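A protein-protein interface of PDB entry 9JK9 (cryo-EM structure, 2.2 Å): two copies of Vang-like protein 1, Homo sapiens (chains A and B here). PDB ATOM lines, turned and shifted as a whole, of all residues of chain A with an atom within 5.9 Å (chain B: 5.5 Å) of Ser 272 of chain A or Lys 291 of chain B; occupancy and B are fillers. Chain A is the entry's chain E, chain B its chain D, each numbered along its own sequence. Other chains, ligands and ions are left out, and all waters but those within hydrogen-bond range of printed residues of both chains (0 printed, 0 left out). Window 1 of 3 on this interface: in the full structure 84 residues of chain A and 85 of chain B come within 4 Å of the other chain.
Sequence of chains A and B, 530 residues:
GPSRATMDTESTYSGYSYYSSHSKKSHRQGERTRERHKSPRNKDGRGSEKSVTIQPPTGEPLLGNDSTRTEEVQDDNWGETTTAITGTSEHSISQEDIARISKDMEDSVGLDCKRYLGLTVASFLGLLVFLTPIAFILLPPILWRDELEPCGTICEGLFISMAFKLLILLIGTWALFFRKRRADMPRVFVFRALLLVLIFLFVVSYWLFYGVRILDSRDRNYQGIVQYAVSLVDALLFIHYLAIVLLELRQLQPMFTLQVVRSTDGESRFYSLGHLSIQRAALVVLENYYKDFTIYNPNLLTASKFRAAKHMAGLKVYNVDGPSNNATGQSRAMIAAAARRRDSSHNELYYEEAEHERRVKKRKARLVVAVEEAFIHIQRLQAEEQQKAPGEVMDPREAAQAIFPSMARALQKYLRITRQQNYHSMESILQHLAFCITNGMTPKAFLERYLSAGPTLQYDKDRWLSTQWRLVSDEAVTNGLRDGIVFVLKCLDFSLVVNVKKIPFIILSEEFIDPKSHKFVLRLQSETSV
OG1 of Thr 257 of chain A lies close to O of Tyr 271 of chain A (3.5 Å).
The side-chain amino group (NZ) of Lys 291 of chain B is in salt-bridge range of the side-chain carboxylate (OD1) of Asp 292 of chain B.
Among the printed residues, merely in contact across the chains: Ser 272 of chain A with Lys 291 of chain B, Phe 270 of chain A with Pro 455 of chain B, Phe 270 of chain A with Lys 291 of chain B and Thr 257 of chain A with Leu 457 of chain B.
Of the printed residues of chain B, Thr 257 of chain A touches Leu 457 (3.6 Å).
Printed residues of chain B within 4 Å of Phe 270 of chain A: Lys 291 and Pro 455.
Ser 272 of chain A touches one residue of chain B.
Of the printed residues of chain A, Pro 455 of chain B touches Phe 270.
Printed residues of chain A within 4 Å of Leu 457 of chain B: Thr 257.
The nearest printed residue of chain A that does not touch Pro 455 of chain B is Thr 257 of chain A (7.7 Å).
Printed residues of chain B that touch a printed residue of chain A: Lys 291, Pro 455 and Leu 457.
Hydrophobic or aromatic side chains of chain B within 4 Å of the printed part of chain A: Pro 455 and Leu 457.
Among the printed residues, 4 pairs touch across the chains.
Among the printed residues, no Asp or Glu carboxylate lies within 4 Å of a Lys or Arg side-chain nitrogen of the other chain.
No position is printed for both chains.
Of the 4 pairs that touch across the chains among the printed residues, none has its exchanged pair printed and touching as well.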
ATOM      1  N   PRO A 254     -22.551  19.763   2.427  1.00  0.00           N
ATOM      2  CA  PRO A 254     -22.858  21.088   2.994  1.00  0.00           C
ATOM      3  C   PRO A 254     -22.994  22.212   1.976  1.00  0.00           C
ATOM      4  O   PRO A 254     -22.013  22.879   1.670  1.00  0.00           O
ATOM      5  CB  PRO A 254     -21.663  21.352   3.919  1.00  0.00           C
ATOM      6  CG  PRO A 254     -21.063  20.018   4.172  1.00  0.00           C
ATOM      7  CD  PRO A 254     -21.258  19.255   2.909  1.00  0.00           C
ATOM      8  N   PHE A 256     -24.698  25.086   2.184  1.00  0.00           N
ATOM      9  CA  PHE A 256     -24.893  26.438   2.685  1.00  0.00           C
ATOM     10  C   PHE A 256     -24.178  26.620   4.009  1.00  0.00           C
ATOM     11  O   PHE A 256     -23.831  25.658   4.690  1.00  0.00           O
ATOM     12  CB  PHE A 256     -26.379  26.755   2.860  1.00  0.00           C
ATOM     13  CG  PHE A 256     -27.145  26.706   1.589  1.00  0.00           C
ATOM     14  CD1 PHE A 256     -27.077  27.755   0.694  1.00  0.00           C
ATOM     15  CD2 PHE A 256     -27.912  25.600   1.273  1.00  0.00           C
ATOM     16  CE1 PHE A 256     -27.759  27.705  -0.486  1.00  0.00           C
ATOM     17  CE2 PHE A 256     -28.604  25.548   0.091  1.00  0.00           C
ATOM     18  CZ  PHE A 256     -28.524  26.602  -0.791  1.00  0.00           C
ATOM     19  N   THR A 257     -23.955  27.878   4.367  1.00  0.00           N
ATOM     20  CA  THR A 257     -23.560  28.234   5.716  1.00  0.00           C
ATOM     21  C   THR A 257     -24.660  29.091   6.329  1.00  0.00           C
ATOM     22  O   THR A 257     -25.435  29.744   5.621  1.00  0.00           O
ATOM     23  CB  THR A 257     -22.207  28.958   5.755  1.00  0.00           C
ATOM     24  OG1 THR A 257     -21.762  29.068   7.110  1.00  0.00           O
ATOM     25  CG2 THR A 257     -22.317  30.342   5.169  1.00  0.00           C
ATOM     26  N   LEU A 258     -24.778  29.028   7.651  1.00  0.00           N
ATOM     27  CA  LEU A 258     -25.848  29.717   8.364  1.00  0.00           C
ATOM     28  C   LEU A 258     -25.242  30.472   9.536  1.00  0.00           C
ATOM     29  O   LEU A 258     -24.662  29.861  10.434  1.00  0.00           O
ATOM     30  CB  LEU A 258     -26.926  28.742   8.848  1.00  0.00           C
ATOM     31  CG  LEU A 258     -28.013  28.250   7.881  1.00  0.00           C
ATOM     32  CD1 LEU A 258     -27.524  27.190   6.907  1.00  0.00           C
ATOM     33  CD2 LEU A 258     -29.202  27.722   8.644  1.00  0.00           C
ATOM     34  N   PHE A 270     -21.586  29.716  13.452  1.00  0.00           N
ATOM     35  CA  PHE A 270     -21.850  29.408  12.055  1.00  0.00           C
ATOM     36  C   PHE A 270     -22.013  27.904  11.890  1.00  0.00           C
ATOM     37  O   PHE A 270     -21.289  27.121  12.511  1.00  0.00           O
ATOM     38  CB  PHE A 270     -20.760  29.870  11.068  1.00  0.00           C
ATOM     39  CG  PHE A 270     -20.645  31.370  10.856  1.00  0.00           C
ATOM     40  CD1 PHE A 270     -21.002  32.299  11.811  1.00  0.00           C
ATOM     41  CD2 PHE A 270     -20.338  31.833   9.590  1.00  0.00           C
ATOM     42  CE1 PHE A 270     -20.894  33.641  11.563  1.00  0.00           C
ATOM     43  CE2 PHE A 270     -20.275  33.181   9.324  1.00  0.00           C
ATOM     44  CZ  PHE A 270     -20.570  34.081  10.310  1.00  0.00           C
ATOM     45  N   TYR A 271     -22.947  27.506  11.035  1.00  0.00           N
ATOM     46  CA  TYR A 271     -23.239  26.101  10.808  1.00  0.00           C
ATOM     47  C   TYR A 271     -23.331  25.835   9.316  1.00  0.00           C
ATOM     48  O   TYR A 271     -23.839  26.667   8.565  1.00  0.00           O
ATOM     49  CB  TYR A 271     -24.545  25.693  11.486  1.00  0.00           C
ATOM     50  CG  TYR A 271     -24.536  25.946  12.967  1.00  0.00           C
ATOM     51  CD1 TYR A 271     -23.816  25.126  13.825  1.00  0.00           C
ATOM     52  CD2 TYR A 271     -25.246  27.005  13.509  1.00  0.00           C
ATOM     53  CE1 TYR A 271     -23.798  25.362  15.180  1.00  0.00           C
ATOM     54  CE2 TYR A 271     -25.241  27.245  14.861  1.00  0.00           C
ATOM     55  CZ  TYR A 271     -24.514  26.422  15.691  1.00  0.00           C
ATOM     56  OH  TYR A 271     -24.510  26.656  17.043  1.00  0.00           O
ATOM     57  N   SER A 272     -22.846  24.675   8.891  1.00  0.00           N
ATOM     58  CA  SER A 272     -22.982  24.236   7.511  1.00  0.00           C
ATOM     59  C   SER A 272     -24.162  23.289   7.369  1.00  0.00           C
ATOM     60  O   SER A 272     -24.335  22.371   8.173  1.00  0.00           O
ATOM     61  CB  SER A 272     -21.713  23.547   7.010  1.00  0.00           C
ATOM     62  OG  SER A 272     -20.667  24.478   6.834  1.00  0.00           O
ATOM     63  N   LEU A 273     -24.974  23.522   6.340  1.00  0.00           N
ATOM     64  CA  LEU A 273     -26.127  22.685   6.055  1.00  0.00           C
ATOM     65  C   LEU A 273     -26.220  22.405   4.566  1.00  0.00           C
ATOM     66  O   LEU A 273     -25.763  23.193   3.736  1.00  0.00           O
ATOM     67  CB  LEU A 273     -27.437  23.321   6.532  1.00  0.00           C
ATOM     68  CG  LEU A 273     -27.653  23.322   8.038  1.00  0.00           C
ATOM     69  CD1 LEU A 273     -28.958  23.989   8.395  1.00  0.00           C
ATOM     70  CD2 LEU A 273     -27.629  21.896   8.522  1.00  0.00           C
ATOM     71  N   GLY A 274     -26.823  21.274   4.242  1.00  0.00           N
ATOM     72  CA  GLY A 274     -27.090  20.895   2.873  1.00  0.00           C
ATOM     73  C   GLY A 274     -28.391  21.460   2.364  1.00  0.00           C
ATOM     74  O   GLY A 274     -28.862  22.505   2.817  1.00  0.00           O
ATOM     75  N   ILE A 503     -22.160  28.469   0.328  1.00  0.00           N
ATOM     76  CA  ILE A 503     -20.721  28.207   0.438  1.00  0.00           C
ATOM     77  C   ILE A 503     -20.084  28.392  -0.931  1.00  0.00           C
ATOM     78  O   ILE A 503     -20.581  27.826  -1.923  1.00  0.00           O
ATOM     79  CB  ILE A 503     -20.469  26.797   1.007  1.00  0.00           C
ATOM     80  CG1 ILE A 503     -20.839  26.788   2.488  1.00  0.00           C
ATOM     81  CG2 ILE A 503     -19.041  26.342   0.796  1.00  0.00           C
ATOM     82  CD1 ILE A 503     -20.742  25.449   3.141  1.00  0.00           C
ATOM     83  N   LEU B 286     -11.344  23.786   3.307  1.00  0.00           N
ATOM     84  CA  LEU B 286     -11.640  25.158   2.897  1.00  0.00           C
ATOM     85  C   LEU B 286     -13.056  25.584   3.272  1.00  0.00           C
ATOM     86  O   LEU B 286     -13.277  26.757   3.606  1.00  0.00           O
ATOM     87  CB  LEU B 286     -11.397  25.335   1.404  1.00  0.00           C
ATOM     88  CG  LEU B 286      -9.905  25.327   1.092  1.00  0.00           C
ATOM     89  CD1 LEU B 286      -9.667  25.472  -0.371  1.00  0.00           C
ATOM     90  CD2 LEU B 286      -9.196  26.422   1.848  1.00  0.00           C
ATOM     91  N   GLU B 287     -14.020  24.653   3.215  1.00  0.00           N
ATOM     92  CA  GLU B 287     -15.365  24.895   3.747  1.00  0.00           C
ATOM     93  C   GLU B 287     -15.299  25.331   5.203  1.00  0.00           C
ATOM     94  O   GLU B 287     -15.845  26.374   5.593  1.00  0.00           O
ATOM     95  CB  GLU B 287     -16.203  23.622   3.657  1.00  0.00           C
ATOM     96  CG  GLU B 287     -16.461  23.068   2.287  1.00  0.00           C
ATOM     97  CD  GLU B 287     -16.976  21.642   2.361  1.00  0.00           C
ATOM     98  OE1 GLU B 287     -17.167  21.142   3.490  1.00  0.00           O
ATOM     99  OE2 GLU B 287     -17.106  20.993   1.304  1.00  0.00           O
ATOM    100  N   ASN B 288     -14.586  24.548   6.008  1.00  0.00           N
ATOM    101  CA  ASN B 288     -14.404  24.873   7.410  1.00  0.00           C
ATOM    102  C   ASN B 288     -13.546  26.114   7.619  1.00  0.00           C
ATOM    103  O   ASN B 288     -13.663  26.747   8.667  1.00  0.00           O
ATOM    104  CB  ASN B 288     -13.796  23.673   8.124  1.00  0.00           C
ATOM    105  CG  ASN B 288     -14.751  22.506   8.205  1.00  0.00           C
ATOM    106  OD1 ASN B 288     -15.934  22.678   8.484  1.00  0.00           O
ATOM    107  ND2 ASN B 288     -14.244  21.308   7.949  1.00  0.00           N
ATOM    108  N   TYR B 289     -12.684  26.464   6.659  1.00  0.00           N
ATOM    109  CA  TYR B 289     -11.925  27.706   6.753  1.00  0.00           C
ATOM    110  C   TYR B 289     -12.844  28.907   6.656  1.00  0.00           C
ATOM    111  O   TYR B 289     -12.737  29.849   7.448  1.00  0.00           O
ATOM    112  CB  TYR B 289     -10.852  27.792   5.659  1.00  0.00           C
ATOM    113  CG  TYR B 289     -10.140  29.129   5.709  1.00  0.00           C
ATOM    114  CD1 TYR B 289      -9.225  29.394   6.709  1.00  0.00           C
ATOM    115  CD2 TYR B 289     -10.413  30.142   4.786  1.00  0.00           C
ATOM    116  CE1 TYR B 289      -8.595  30.606   6.796  1.00  0.00           C
ATOM    117  CE2 TYR B 289      -9.789  31.368   4.876  1.00  0.00           C
ATOM    118  CZ  TYR B 289      -8.878  31.586   5.884  1.00  0.00           C
ATOM    119  OH  TYR B 289      -8.239  32.790   6.007  1.00  0.00           O
ATOM    120  N   TYR B 290     -13.723  28.909   5.655  1.00  0.00           N
ATOM    121  CA  TYR B 290     -14.642  30.029   5.504  1.00  0.00           C
ATOM    122  C   TYR B 290     -15.670  30.075   6.628  1.00  0.00           C
ATOM    123  O   TYR B 290     -16.161  31.154   6.969  1.00  0.00           O
ATOM    124  CB  TYR B 290     -15.323  29.979   4.140  1.00  0.00           C
ATOM    125  CG  TYR B 290     -14.395  30.343   3.022  1.00  0.00           C
ATOM    126  CD1 TYR B 290     -13.980  31.652   2.853  1.00  0.00           C
ATOM    127  CD2 TYR B 290     -13.951  29.391   2.119  1.00  0.00           C
ATOM    128  CE1 TYR B 290     -13.125  31.993   1.843  1.00  0.00           C
ATOM    129  CE2 TYR B 290     -13.097  29.727   1.100  1.00  0.00           C
ATOM    130  CZ  TYR B 290     -12.692  31.033   0.967  1.00  0.00           C
ATOM    131  OH  TYR B 290     -11.842  31.393  -0.043  1.00  0.00           O
ATOM    132  N   LYS B 291     -15.980  28.931   7.236  1.00  0.00           N
ATOM    133  CA  LYS B 291     -16.929  28.938   8.344  1.00  0.00           C
ATOM    134  C   LYS B 291     -16.283  29.295   9.687  1.00  0.00           C
ATOM    135  O   LYS B 291     -16.913  29.971  10.506  1.00  0.00           O
ATOM    136  CB  LYS B 291     -17.609  27.570   8.426  1.00  0.00           C
ATOM    137  CG  LYS B 291     -18.629  27.414   9.520  1.00  0.00           C
ATOM    138  CD  LYS B 291     -19.332  26.088   9.426  1.00  0.00           C
ATOM    139  CE  LYS B 291     -18.414  24.946   9.798  1.00  0.00           C
ATOM    140  NZ  LYS B 291     -18.098  24.955  11.248  1.00  0.00           N
ATOM    141  N   ASP B 292     -15.034  28.901   9.923  1.00  0.00           N
ATOM    142  CA  ASP B 292     -14.508  28.750  11.278  1.00  0.00           C
ATOM    143  C   ASP B 292     -13.360  29.683  11.631  1.00  0.00           C
ATOM    144  O   ASP B 292     -13.341  30.228  12.735  1.00  0.00           O
ATOM    145  CB  ASP B 292     -14.053  27.302  11.490  1.00  0.00           C
ATOM    146  CG  ASP B 292     -15.210  26.336  11.636  1.00  0.00           C
ATOM    147  OD1 ASP B 292     -16.275  26.746  12.144  1.00  0.00           O
ATOM    148  OD2 ASP B 292     -15.053  25.161  11.249  1.00  0.00           O
ATOM    149  N   PHE B 293     -12.389  29.859  10.745  1.00  0.00           N
ATOM    150  CA  PHE B 293     -11.245  30.720  11.015  1.00  0.00           C
ATOM    151  C   PHE B 293     -11.654  32.178  10.911  1.00  0.00           C
ATOM    152  O   PHE B 293     -12.476  32.537  10.064  1.00  0.00           O
ATOM    153  CB  PHE B 293     -10.130  30.445  10.010  1.00  0.00           C
ATOM    154  CG  PHE B 293      -9.406  29.146  10.216  1.00  0.00           C
ATOM    155  CD1 PHE B 293      -8.185  29.115  10.860  1.00  0.00           C
ATOM    156  CD2 PHE B 293      -9.967  27.950   9.802  1.00  0.00           C
ATOM    157  CE1 PHE B 293      -7.525  27.923  11.041  1.00  0.00           C
ATOM    158  CE2 PHE B 293      -9.314  26.759   9.996  1.00  0.00           C
ATOM    159  CZ  PHE B 293      -8.092  26.746  10.617  1.00  0.00           C
ATOM    160  N   PRO B 455     -15.528  35.378  11.363  1.00  0.00           N
ATOM    161  CA  PRO B 455     -15.061  34.518  10.275  1.00  0.00           C
ATOM    162  C   PRO B 455     -15.188  35.187   8.914  1.00  0.00           C
ATOM    163  O   PRO B 455     -15.720  36.287   8.769  1.00  0.00           O
ATOM    164  CB  PRO B 455     -15.963  33.286  10.381  1.00  0.00           C
ATOM    165  CG  PRO B 455     -17.160  33.772  11.052  1.00  0.00           C
ATOM    166  CD  PRO B 455     -16.747  34.851  11.990  1.00  0.00           C
ATOM    167  N   LEU B 457     -16.790  34.531   6.116  1.00  0.00           N
ATOM    168  CA  LEU B 457     -18.071  34.679   5.437  1.00  0.00           C
ATOM    169  C   LEU B 457     -18.964  35.772   6.013  1.00  0.00           C
ATOM    170  O   LEU B 457     -20.040  36.002   5.456  1.00  0.00           O
ATOM    171  CB  LEU B 457     -18.822  33.350   5.450  1.00  0.00           C
ATOM    172  CG  LEU B 457     -18.177  32.318   4.534  1.00  0.00           C
ATOM    173  CD1 LEU B 457     -18.787  30.962   4.746  1.00  0.00           C
ATOM    174  CD2 LEU B 457     -18.312  32.735   3.081  1.00  0.00           C
